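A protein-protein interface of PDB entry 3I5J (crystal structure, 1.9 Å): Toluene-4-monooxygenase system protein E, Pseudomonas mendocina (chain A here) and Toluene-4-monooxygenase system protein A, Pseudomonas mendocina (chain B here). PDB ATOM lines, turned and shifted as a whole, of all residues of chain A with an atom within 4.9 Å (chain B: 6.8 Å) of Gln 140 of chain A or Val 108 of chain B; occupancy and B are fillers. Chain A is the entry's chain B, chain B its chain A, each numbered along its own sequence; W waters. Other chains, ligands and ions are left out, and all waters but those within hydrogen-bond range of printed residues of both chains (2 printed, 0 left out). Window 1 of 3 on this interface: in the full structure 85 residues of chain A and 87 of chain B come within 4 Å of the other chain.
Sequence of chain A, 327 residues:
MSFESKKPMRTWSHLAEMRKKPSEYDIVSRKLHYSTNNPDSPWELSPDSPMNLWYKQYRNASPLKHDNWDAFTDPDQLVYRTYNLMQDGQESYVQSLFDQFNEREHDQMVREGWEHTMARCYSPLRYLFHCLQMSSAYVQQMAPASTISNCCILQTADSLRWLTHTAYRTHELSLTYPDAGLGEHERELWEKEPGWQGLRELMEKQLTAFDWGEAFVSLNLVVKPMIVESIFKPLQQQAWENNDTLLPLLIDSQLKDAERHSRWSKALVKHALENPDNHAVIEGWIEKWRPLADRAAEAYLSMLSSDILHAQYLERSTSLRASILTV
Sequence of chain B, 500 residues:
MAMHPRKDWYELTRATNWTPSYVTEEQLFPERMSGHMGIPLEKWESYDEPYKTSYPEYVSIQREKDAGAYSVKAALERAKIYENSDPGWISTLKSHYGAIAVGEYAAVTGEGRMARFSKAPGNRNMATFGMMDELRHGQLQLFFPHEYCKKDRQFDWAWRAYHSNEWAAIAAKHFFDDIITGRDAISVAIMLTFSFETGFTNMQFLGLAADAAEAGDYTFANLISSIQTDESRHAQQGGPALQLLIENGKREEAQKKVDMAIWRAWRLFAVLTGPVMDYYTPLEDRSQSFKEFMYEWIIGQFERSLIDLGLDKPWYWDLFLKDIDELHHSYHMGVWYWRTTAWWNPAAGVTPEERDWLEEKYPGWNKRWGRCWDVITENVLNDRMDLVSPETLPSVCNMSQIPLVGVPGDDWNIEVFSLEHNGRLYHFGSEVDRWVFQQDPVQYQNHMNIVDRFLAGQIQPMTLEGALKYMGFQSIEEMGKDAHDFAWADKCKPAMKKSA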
ATOM      1  N   HIS A  33      28.890   2.543  -5.749  1.00  0.00           N
ATOM      2  CA  HIS A  33      28.693   3.523  -4.675  1.00  0.00           C
ATOM      3  C   HIS A  33      30.012   3.975  -4.098  1.00  0.00           C
ATOM      4  O   HIS A  33      30.539   3.290  -3.292  1.00  0.00           O
ATOM      5  CB  HIS A  33      27.909   2.963  -3.484  1.00  0.00           C
ATOM      6  CG  HIS A  33      26.449   2.659  -3.761  1.00  0.00           C
ATOM      7  ND1 HIS A  33      25.688   3.365  -4.665  1.00  0.00           N
ATOM      8  CD2 HIS A  33      25.597   1.812  -3.144  1.00  0.00           C
ATOM      9  CE1 HIS A  33      24.428   2.969  -4.606  1.00  0.00           C
ATOM     10  NE2 HIS A  33      24.358   1.977  -3.743  1.00  0.00           N
ATOM     11  N   SER A 136      10.561   0.987  -1.918  1.00  0.00           N
ATOM     12  CA  SER A 136      11.680   0.473  -2.735  1.00  0.00           C
ATOM     13  C   SER A 136      12.714   1.526  -3.052  1.00  0.00           C
ATOM     14  O   SER A 136      13.929   1.232  -3.089  1.00  0.00           O
ATOM     15  CB  SER A 136      11.199  -0.154  -4.098  1.00  0.00           C
ATOM     16  OG  SER A 136      10.204  -1.144  -3.801  1.00  0.00           O
ATOM     17  N   ALA A 137      12.243   2.733  -3.340  1.00  0.00           N
ATOM     18  CA  ALA A 137      13.168   3.842  -3.648  1.00  0.00           C
ATOM     19  C   ALA A 137      14.024   4.169  -2.458  1.00  0.00           C
ATOM     20  O   ALA A 137      15.217   4.553  -2.546  1.00  0.00           O
ATOM     21  CB  ALA A 137      12.361   5.114  -4.199  1.00  0.00           C
ATOM     22  N   TYR A 138      13.429   3.970  -1.292  1.00  0.00           N
ATOM     23  CA  TYR A 138      14.232   4.223  -0.070  1.00  0.00           C
ATOM     24  C   TYR A 138      15.332   3.155   0.097  1.00  0.00           C
ATOM     25  O   TYR A 138      16.518   3.479   0.403  1.00  0.00           O
ATOM     26  CB  TYR A 138      13.347   4.364   1.214  1.00  0.00           C
ATOM     27  CG  TYR A 138      14.233   4.767   2.394  1.00  0.00           C
ATOM     28  CD1 TYR A 138      14.613   3.814   3.366  1.00  0.00           C
ATOM     29  CD2 TYR A 138      14.766   6.073   2.482  1.00  0.00           C
ATOM     30  CE1 TYR A 138      15.459   4.190   4.463  1.00  0.00           C
ATOM     31  CE2 TYR A 138      15.609   6.454   3.557  1.00  0.00           C
ATOM     32  CZ  TYR A 138      15.957   5.503   4.523  1.00  0.00           C
ATOM     33  OH  TYR A 138      16.836   5.866   5.538  1.00  0.00           O
ATOM     34  N   VAL A 139      14.987   1.884  -0.053  1.00  0.00           N
ATOM     35  CA  VAL A 139      16.063   0.872   0.056  1.00  0.00           C
ATOM     36  C   VAL A 139      17.156   1.135  -1.003  1.00  0.00           C
ATOM     37  O   VAL A 139      18.349   1.073  -0.692  1.00  0.00           O
ATOM     38  CB  VAL A 139      15.488  -0.591   0.014  1.00  0.00           C
ATOM     39  CG1 VAL A 139      16.556  -1.684   0.265  1.00  0.00           C
ATOM     40  CG2 VAL A 139      14.305  -0.797   1.021  1.00  0.00           C
ATOM     41  N   GLN A 140      16.756   1.513  -2.227  1.00  0.00           N
ATOM     42  CA  GLN A 140      17.711   1.899  -3.280  1.00  0.00           C
ATOM     43  C   GLN A 140      18.748   2.918  -2.793  1.00  0.00           C
ATOM     44  O   GLN A 140      19.968   2.779  -2.997  1.00  0.00           O
ATOM     45  CB  GLN A 140      16.963   2.463  -4.521  1.00  0.00           C
ATOM     46  CG  GLN A 140      17.890   3.174  -5.595  1.00  0.00           C
ATOM     47  CD  GLN A 140      18.310   4.609  -5.243  1.00  0.00           C
ATOM     48  OE1 GLN A 140      17.477   5.459  -4.910  1.00  0.00           O
ATOM     49  NE2 GLN A 140      19.628   4.892  -5.323  1.00  0.00           N
ATOM     50  N   GLN A 141      18.249   3.989  -2.191  1.00  0.00           N
ATOM     51  CA  GLN A 141      19.144   5.062  -1.971  1.00  0.00           C
ATOM     52  C   GLN A 141      20.042   4.740  -0.753  1.00  0.00           C
ATOM     53  O   GLN A 141      21.108   5.366  -0.649  1.00  0.00           O
ATOM     54  CB  GLN A 141      18.422   6.417  -1.732  1.00  0.00           C
ATOM     55  CG  GLN A 141      17.473   6.470  -0.445  1.00  0.00           C
ATOM     56  CD  GLN A 141      16.344   7.484  -0.757  1.00  0.00           C
ATOM     57  OE1 GLN A 141      15.473   7.235  -1.657  1.00  0.00           O
ATOM     58  NE2 GLN A 141      16.406   8.643  -0.120  1.00  0.00           N
ATOM     59  N   MET A 142      19.587   3.857   0.137  1.00  0.00           N
ATOM     60  CA  MET A 142      20.338   3.566   1.373  1.00  0.00           C
ATOM     61  C   MET A 142      21.180   2.283   1.285  1.00  0.00           C
ATOM     62  O   MET A 142      22.074   2.048   2.096  1.00  0.00           O
ATOM     63  CB  MET A 142      19.402   3.434   2.574  1.00  0.00           C
ATOM     64  CG  MET A 142      18.651   4.749   2.911  1.00  0.00           C
ATOM     65  SD  MET A 142      19.643   6.286   2.967  1.00  0.00           S
ATOM     66  CE  MET A 142      20.837   5.805   4.242  1.00  0.00           C
ATOM     67  N   ALA A 143      20.891   1.411   0.350  1.00  0.00           N
ATOM     68  CA  ALA A 143      21.632   0.110   0.351  1.00  0.00           C
ATOM     69  C   ALA A 143      23.167   0.269   0.151  1.00  0.00           C
ATOM     70  O   ALA A 143      23.638   1.174  -0.569  1.00  0.00           O
ATOM     71  CB  ALA A 143      21.026  -0.878  -0.679  1.00  0.00           C
ATOM     72  N   SER A 149      21.332  -1.933  -4.769  1.00  0.00           N
ATOM     73  CA  SER A 149      20.518  -0.773  -5.174  1.00  0.00           C
ATOM     74  C   SER A 149      19.862  -0.947  -6.563  1.00  0.00           C
ATOM     75  O   SER A 149      18.722  -0.548  -6.767  1.00  0.00           O
ATOM     76  CB  SER A 149      21.339   0.520  -5.223  1.00  0.00           C
ATOM     77  OG  SER A 149      21.701   0.921  -3.929  1.00  0.00           O
ATOM     78  N   CYS A 152      16.746  -2.798  -6.274  1.00  0.00           N
ATOM     79  CA  CYS A 152      15.708  -1.906  -5.752  1.00  0.00           C
ATOM     80  C   CYS A 152      15.182  -0.945  -6.801  1.00  0.00           C
ATOM     81  O   CYS A 152      14.000  -0.580  -6.735  1.00  0.00           O
ATOM     82  CB  CYS A 152      16.221  -1.081  -4.562  1.00  0.00           C
ATOM     83  SG  CYS A 152      16.688  -2.195  -3.179  1.00  0.00           S
ATOM     84  N   ILE A 153      16.064  -0.415  -7.641  1.00  0.00           N
ATOM     85  CA  ILE A 153      15.560   0.493  -8.648  1.00  0.00           C
ATOM     86  C   ILE A 153      14.494  -0.217  -9.513  1.00  0.00           C
ATOM     87  O   ILE A 153      13.391   0.328  -9.835  1.00  0.00           O
ATOM     88  CB  ILE A 153      16.680   1.043  -9.586  1.00  0.00           C
ATOM     89  CG1 ILE A 153      17.746   1.896  -8.824  1.00  0.00           C
ATOM     90  CG2 ILE A 153      16.053   1.813 -10.808  1.00  0.00           C
ATOM     91  CD1 ILE A 153      19.098   1.937  -9.564  1.00  0.00           C
ATOM     92  N   GLY B 103      28.971   9.631 -11.747  1.00  0.00           N
ATOM     93  CA  GLY B 103      28.145  10.811 -11.332  1.00  0.00           C
ATOM     94  C   GLY B 103      26.661  10.591 -11.825  1.00  0.00           C
ATOM     95  O   GLY B 103      25.715  10.868 -11.090  1.00  0.00           O
ATOM     96  N   GLU B 104      26.457  10.043 -13.018  1.00  0.00           N
ATOM     97  CA  GLU B 104      25.114   9.639 -13.498  1.00  0.00           C
ATOM     98  C   GLU B 104      24.535   8.633 -12.557  1.00  0.00           C
ATOM     99  O   GLU B 104      23.404   8.696 -12.181  1.00  0.00           O
ATOM    100  CB  GLU B 104      25.166   8.981 -14.870  1.00  0.00           C
ATOM    101  CG  GLU B 104      25.763   9.855 -16.021  1.00  0.00           C
ATOM    102  CD  GLU B 104      24.705  10.654 -16.665  1.00  0.00           C
ATOM    103  OE1 GLU B 104      24.924  11.237 -17.759  1.00  0.00           O
ATOM    104  OE2 GLU B 104      23.641  10.721 -16.009  1.00  0.00           O
ATOM    105  N   TYR B 105      25.313   7.617 -12.214  1.00  0.00           N
ATOM    106  CA  TYR B 105      24.801   6.627 -11.293  1.00  0.00           C
ATOM    107  C   TYR B 105      24.447   7.258  -9.904  1.00  0.00           C
ATOM    108  O   TYR B 105      23.455   6.863  -9.213  1.00  0.00           O
ATOM    109  CB  TYR B 105      25.797   5.442 -11.125  1.00  0.00           C
ATOM    110  CG  TYR B 105      25.164   4.344 -10.291  1.00  0.00           C
ATOM    111  CD1 TYR B 105      24.191   3.529 -10.851  1.00  0.00           C
ATOM    112  CD2 TYR B 105      25.505   4.153  -8.948  1.00  0.00           C
ATOM    113  CE1 TYR B 105      23.555   2.519 -10.091  1.00  0.00           C
ATOM    114  CE2 TYR B 105      24.909   3.141  -8.176  1.00  0.00           C
ATOM    115  CZ  TYR B 105      23.907   2.361  -8.741  1.00  0.00           C
ATOM    116  OH  TYR B 105      23.233   1.365  -8.040  1.00  0.00           O
ATOM    117  N   ALA B 106      25.248   8.233  -9.458  1.00  0.00           N
ATOM    118  CA  ALA B 106      24.881   9.026  -8.207  1.00  0.00           C
ATOM    119  C   ALA B 106      23.534   9.731  -8.382  1.00  0.00           C
ATOM    120  O   ALA B 106      22.745   9.861  -7.423  1.00  0.00           O
ATOM    121  CB  ALA B 106      25.955  10.010  -7.814  1.00  0.00           C
ATOM    122  N   ALA B 107      23.277  10.188  -9.616  1.00  0.00           N
ATOM    123  CA  ALA B 107      22.041  10.903  -9.822  1.00  0.00           C
ATOM    124  C   ALA B 107      20.809  10.006  -9.594  1.00  0.00           C
ATOM    125  O   ALA B 107      19.716  10.538  -9.361  1.00  0.00           O
ATOM    126  CB  ALA B 107      21.976  11.555 -11.252  1.00  0.00           C
ATOM    127  N   VAL B 108      20.951   8.667  -9.760  1.00  0.00           N
ATOM    128  CA  VAL B 108      19.861   7.762  -9.360  1.00  0.00           C
ATOM    129  C   VAL B 108      19.373   8.112  -7.949  1.00  0.00           C
ATOM    130  O   VAL B 108      18.186   8.038  -7.668  1.00  0.00           O
ATOM    131  CB  VAL B 108      20.254   6.287  -9.379  1.00  0.00           C
ATOM    132  CG1 VAL B 108      19.090   5.459  -8.804  1.00  0.00           C
ATOM    133  CG2 VAL B 108      20.647   5.821 -10.817  1.00  0.00           C
ATOM    134  N   THR B 109      20.334   8.391  -7.042  1.00  0.00           N
ATOM    135  CA  THR B 109      20.039   8.690  -5.655  1.00  0.00           C
ATOM    136  C   THR B 109      19.347  10.070  -5.494  1.00  0.00           C
ATOM    137  O   THR B 109      18.483  10.220  -4.668  1.00  0.00           O
ATOM    138  CB  THR B 109      21.337   8.606  -4.780  1.00  0.00           C
ATOM    139  OG1 THR B 109      21.702   7.227  -4.665  1.00  0.00           O
ATOM    140  CG2 THR B 109      21.159   9.268  -3.388  1.00  0.00           C
ATOM    141  N   GLY B 110      19.665  11.070  -6.307  1.00  0.00           N
ATOM    142  CA  GLY B 110      18.846  12.348  -6.228  1.00  0.00           C
ATOM    143  C   GLY B 110      17.411  12.012  -6.644  1.00  0.00           C
ATOM    144  O   GLY B 110      16.435  12.487  -6.035  1.00  0.00           O
ATOM    145  N   GLU B 111      17.234  11.207  -7.697  1.00  0.00           N
ATOM    146  CA  GLU B 111      15.872  10.868  -8.169  1.00  0.00           C
ATOM    147  C   GLU B 111      15.186   9.983  -7.150  1.00  0.00           C
ATOM    148  O   GLU B 111      14.033  10.200  -6.832  1.00  0.00           O
ATOM    149  CB  GLU B 111      15.917  10.185  -9.513  1.00  0.00           C
ATOM    150  CG  GLU B 111      16.474  11.151 -10.601  1.00  0.00           C
ATOM    151  CD  GLU B 111      15.418  12.177 -11.117  1.00  0.00           C
ATOM    152  OE1 GLU B 111      14.226  12.034 -10.855  1.00  0.00           O
ATOM    153  OE2 GLU B 111      15.773  13.170 -11.792  1.00  0.00           O
ATOM    154  N   GLY B 112      15.931   9.110  -6.493  1.00  0.00           N
ATOM    155  CA  GLY B 112      15.291   8.275  -5.447  1.00  0.00           C
ATOM    156  C   GLY B 112      14.842   9.064  -4.217  1.00  0.00           C
ATOM    157  O   GLY B 112      13.851   8.681  -3.516  1.00  0.00           O
ATOM    158  N   ARG B 113      15.656  10.083  -3.878  1.00  0.00           N
ATOM    159  CA  ARG B 113      15.321  11.036  -2.811  1.00  0.00           C
ATOM    160  C   ARG B 113      13.932  11.652  -3.067  1.00  0.00           C
ATOM    161  O   ARG B 113      13.092  11.770  -2.158  1.00  0.00           O
ATOM    162  CB  ARG B 113      16.402  12.127  -2.654  1.00  0.00           C
ATOM    163  CG  ARG B 113      16.394  12.808  -1.227  1.00  0.00           C
ATOM    164  CD  ARG B 113      17.123  11.928  -0.208  1.00  0.00           C
ATOM    165  NE  ARG B 113      18.594  11.929  -0.520  1.00  0.00           N
ATOM    166  CZ  ARG B 113      19.396  10.884  -0.269  1.00  0.00           C
ATOM    167  NH1 ARG B 113      18.969   9.758   0.331  1.00  0.00           N
ATOM    168  NH2 ARG B 113      20.652  10.981  -0.543  1.00  0.00           N
ATOM    169  N   ALA B 127       9.961  10.908 -10.742  1.00  0.00           N
ATOM    170  CA  ALA B 127      11.294  10.595 -10.182  1.00  0.00           C
ATOM    171  C   ALA B 127      11.638   9.112 -10.346  1.00  0.00           C
ATOM    172  O   ALA B 127      12.765   8.750 -10.313  1.00  0.00           O
ATOM    173  CB  ALA B 127      11.384  11.023  -8.693  1.00  0.00           C
ATOM    174  N   GLY B 130      12.878   8.894 -13.570  1.00  0.00           N
ATOM    175  CA  GLY B 130      14.217   9.573 -13.463  1.00  0.00           C
ATOM    176  C   GLY B 130      15.253   8.607 -12.895  1.00  0.00           C
ATOM    177  O   GLY B 130      16.419   8.652 -13.311  1.00  0.00           O
ATOM    178  N   MET B 131      14.872   7.790 -11.889  1.00  0.00           N
ATOM    179  CA  MET B 131      15.794   6.836 -11.335  1.00  0.00           C
ATOM    180  C   MET B 131      16.253   5.899 -12.441  1.00  0.00           C
ATOM    181  O   MET B 131      17.413   5.519 -12.550  1.00  0.00           O
ATOM    182  CB  MET B 131      15.104   6.028 -10.242  1.00  0.00           C
ATOM    183  CG  MET B 131      14.874   6.773  -8.914  1.00  0.00           C
ATOM    184  SD  MET B 131      13.754   5.827  -7.797  1.00  0.00           S
ATOM    185  CE  MET B 131      14.837   4.460  -7.232  1.00  0.00           C
ATOM    186  N   MET B 132      15.283   5.415 -13.170  1.00  0.00           N
ATOM    187  CA  MET B 132      15.534   4.497 -14.262  1.00  0.00           C
ATOM    188  C   MET B 132      16.391   5.149 -15.333  1.00  0.00           C
ATOM    189  O   MET B 132      17.333   4.542 -15.824  1.00  0.00           O
ATOM    190  CB  MET B 132      14.169   4.013 -14.842  1.00  0.00           C
ATOM    191  CG  MET B 132      13.427   3.072 -13.866  1.00  0.00           C
ATOM    192  SD  MET B 132      14.295   1.430 -13.893  1.00  0.00           S
ATOM    193  CE  MET B 132      13.845   0.797 -15.514  1.00  0.00           C
ATOM    194  N   ASP B 133      16.053   6.379 -15.711  1.00  0.00           N
ATOM    195  CA  ASP B 133      16.909   7.062 -16.666  1.00  0.00           C
ATOM    196  C   ASP B 133      18.399   7.155 -16.228  1.00  0.00           C
ATOM    197  O   ASP B 133      19.277   6.985 -17.049  1.00  0.00           O
ATOM    198  CB  ASP B 133      16.443   8.487 -16.899  1.00  0.00           C
ATOM    199  CG  ASP B 133      15.039   8.590 -17.542  1.00  0.00           C
ATOM    200  OD1 ASP B 133      14.595   7.639 -18.237  1.00  0.00           O
ATOM    201  OD2 ASP B 133      14.384   9.666 -17.352  1.00  0.00           O
ATOM    202  N   GLU B 134      18.669   7.563 -15.003  1.00  0.00           N
ATOM    203  CA  GLU B 134      20.049   7.754 -14.596  1.00  0.00           C
ATOM    204  C   GLU B 134      20.750   6.385 -14.509  1.00  0.00           C
ATOM    205  O   GLU B 134      21.955   6.287 -14.722  1.00  0.00           O
ATOM    206  CB  GLU B 134      20.178   8.487 -13.252  1.00  0.00           C
ATOM    207  CG  GLU B 134      19.487   9.910 -13.244  1.00  0.00           C
ATOM    208  CD  GLU B 134      20.014  10.885 -14.292  1.00  0.00           C
ATOM    209  OE1 GLU B 134      20.880  10.543 -15.164  1.00  0.00           O
ATOM    210  OE2 GLU B 134      19.511  12.044 -14.225  1.00  0.00           O
ATOM    211  N   LEU B 135      20.002   5.352 -14.159  1.00  0.00           N
ATOM    212  CA  LEU B 135      20.543   4.004 -14.208  1.00  0.00           C
ATOM    213  C   LEU B 135      21.033   3.740 -15.651  1.00  0.00           C
ATOM    214  O   LEU B 135      22.136   3.304 -15.849  1.00  0.00           O
ATOM    215  CB  LEU B 135      19.522   2.961 -13.799  1.00  0.00           C
ATOM    216  CG  LEU B 135      19.993   1.511 -13.849  1.00  0.00           C
ATOM    217  CD1 LEU B 135      21.189   1.262 -12.877  1.00  0.00           C
ATOM    218  CD2 LEU B 135      18.871   0.581 -13.515  1.00  0.00           C
ATOM    219  N   ARG B 136      20.172   3.971 -16.633  1.00  0.00           N
ATOM    220  CA  ARG B 136      20.585   3.873 -18.027  1.00  0.00           C
ATOM    221  C   ARG B 136      21.882   4.637 -18.316  1.00  0.00           C
ATOM    222  O   ARG B 136      22.801   4.165 -18.978  1.00  0.00           O
ATOM    223  CB  ARG B 136      19.414   4.393 -18.902  1.00  0.00           C
ATOM    224  CG  ARG B 136      19.793   4.444 -20.393  1.00  0.00           C
ATOM    225  CD  ARG B 136      18.736   5.194 -21.326  1.00  0.00           C
ATOM    226  NE  ARG B 136      19.095   4.848 -22.731  1.00  0.00           N
ATOM    227  CZ  ARG B 136      19.186   5.732 -23.702  1.00  0.00           C
ATOM    228  NH1 ARG B 136      18.878   7.019 -23.449  1.00  0.00           N
ATOM    229  NH2 ARG B 136      19.604   5.336 -24.885  1.00  0.00           N
ATOM    230  N   GLY B 138      24.218   5.821 -16.341  1.00  0.00           N
ATOM    231  CA  GLY B 138      25.398   5.270 -15.640  1.00  0.00           C
ATOM    232  C   GLY B 138      25.878   4.001 -16.410  1.00  0.00           C
ATOM    233  O   GLY B 138      27.117   3.823 -16.655  1.00  0.00           O
ATOM    234  N   ILE B 180      23.046  16.873  -5.587  1.00  0.00           N
ATOM    235  CA  ILE B 180      22.284  15.702  -5.972  1.00  0.00           C
ATOM    236  C   ILE B 180      22.024  14.801  -4.767  1.00  0.00           C
ATOM    237  O   ILE B 180      20.901  14.466  -4.508  1.00  0.00           O
ATOM    238  CB  ILE B 180      23.011  14.898  -7.088  1.00  0.00           C
ATOM    239  CG1 ILE B 180      23.186  15.754  -8.324  1.00  0.00           C
ATOM    240  CG2 ILE B 180      22.275  13.592  -7.404  1.00  0.00           C
ATOM    241  CD1 ILE B 180      23.708  14.778  -9.484  1.00  0.00           C
ATOM    242  N   THR B 181      23.076  14.409  -4.055  1.00  0.00           N
ATOM    243  CA  THR B 181      22.931  13.326  -3.090  1.00  0.00           C
ATOM    244  C   THR B 181      22.889  13.840  -1.650  1.00  0.00           C
ATOM    245  O   THR B 181      22.539  13.074  -0.712  1.00  0.00           O
ATOM    246  CB  THR B 181      24.080  12.306  -3.216  1.00  0.00           C
ATOM    247  OG1 THR B 181      25.343  12.955  -2.926  1.00  0.00           O
ATOM    248  CG2 THR B 181      24.114  11.650  -4.630  1.00  0.00           C
ATOM    249  N   LEU B 192      19.120  20.246  -8.976  1.00  0.00           N
ATOM    250  CA  LEU B 192      19.513  19.253 -10.034  1.00  0.00           C
ATOM    251  C   LEU B 192      18.579  19.381 -11.239  1.00  0.00           C
ATOM    252  O   LEU B 192      19.011  19.746 -12.364  1.00  0.00           O
ATOM    253  CB  LEU B 192      19.521  17.844  -9.500  1.00  0.00           C
ATOM    254  CG  LEU B 192      19.687  16.717 -10.557  1.00  0.00           C
ATOM    255  CD1 LEU B 192      21.017  16.879 -11.218  1.00  0.00           C
ATOM    256  CD2 LEU B 192      19.509  15.275  -9.953  1.00  0.00           C
HETATM  257  O   HOH W   1      22.801   6.468  -2.327  1.00  0.00           O
HETATM  258  O   HOH W   2      21.789   3.497  -6.658  1.00  0.00           O
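Of the printed residues of chain B, His 33 of chain A touches Tyr 105 (3.6 Å).
Of chain B, only Val 108, Thr 109, Gly 112 and Met 131 come within 4 Å of Gln 140 of chain A.
Of the printed residues of chain B, Ile 153 of chain A touches Val 108, Met 132 and Leu 135.
Printed residues of chain A within 4 Å of Tyr 105 of chain B: His 33 (3.6 Å) and Ser 149 (3.5 Å).
Val 108 of chain B touches just these residues of chain A: Gln 140 (3.6 Å) and Ile 153 (3.6 Å).
Of the printed residues of chain A, Thr 109 of chain B touches Gln 140.
Thr 181 of chain B touches none of the printed residues of chain A.
The nearest residue of chain B that does not touch Gln 140 of chain A is Arg 113 of chain B (5.1 Å).
The nearest printed residue of chain A that does not touch Val 108 of chain B is Gln 141 of chain A (6.2 Å).
The nearest printed residue of chain A that does not touch Tyr 105 of chain B is Ile 153 of chain A (4.4 Å).
Of the 12 printed residues of chain A, 6 touch a printed residue of chain B.
Hydrophobic or aromatic side chains of chain A that line the printed part of chain B: His 33, Ala 137 and Ile 153.
Along chain A the printed residues that touch a printed residue of chain B span positions 33 to 153.
Hydrophobic or aromatic side chains of chain B that line the printed part of chain A: Tyr 105, Val 108, Met 131, Met 132 and Leu 135.
Among the printed residues, 13 pairs touch across the chains.
Among the printed residues, no Asp or Glu carboxylate lies within 4 Å of a Lys or Arg side-chain nitrogen of the other chain.
Water W1 lies within hydrogen-bond range of O of Gln 141 of chain A and OG1 of Thr 109 of chain B.
Water W2 lies within hydrogen-bond range of NE2 of Gln 140 of chain A and OH of Tyr 105 of chain B.
The backbone carbonyl oxygen (O) of Thr 181 of chain B lies within hydrogen-bond range of the guanidinium group (NH2) of Arg 113 of chain B.
O of Ala 143 of chain A sits close to NE2 of His 33 of chain A.
A ring nitrogen (NE2) of His 33 of chain A is in hydrogen-bond range of the side-chain hydroxyl (OG) of Ser 149 of chain A.
The backbone carbonyl oxygen (O) of Ala 137 of chain A sits close to the side-chain amide oxygen (OE1) of Gln 140 of chain A, 3.4 Å away.
The backbone carbonyl oxygen (O) of Ala 137 of chain A sits close to the side-chain amide oxygen (OE1) of Gln 141 of chain A (2.8 Å).
O of Gln 140 of chain A sits at hydrogen-bond distance from OG of Ser 149 of chain A (2.7 Å).
NE2 of Gln 140 of chain A lies within hydrogen-bond range of OG1 of Thr 109 of chain B.
The side-chain amide oxygen (OE1) of Gln 141 of chain A sits close to the backbone carbonyl oxygen (O) of Gly 112 of chain B.
NH1 of Arg 113 of chain B sits close to NE2 of Gln 141 of chain A, at 2.8 Å.
ND1 of His 33 of chain A touches CE2 of Tyr 105 of chain B, at 3.6 Å.
Gly 112 of chain B touches Ala 137 of chain A (O to CB, 3.9 Å).
CB of Ala 137 of chain A touches SD of Met 131 of chain B, at 3.9 Å.
Val 108 of chain B touches Gln 140 of chain A.
Gln 140 of chain A touches Gly 112 of chain B (OE1 to CA, 3.6 Å).
Gln 140 of chain A touches Met 131 of chain B.
CB of Ser 149 of chain A touches OH of Tyr 105 of chain B, 3.5 Å away.
Ile 153 of chain A touches Val 108 of chain B (CD1 to CG1, 3.6 Å).
Met 132 of chain B touches Ile 153 of chain A.
CD1 of Ile 153 of chain A touches CD1 of Leu 135 of chain B, at 3.98 Å.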
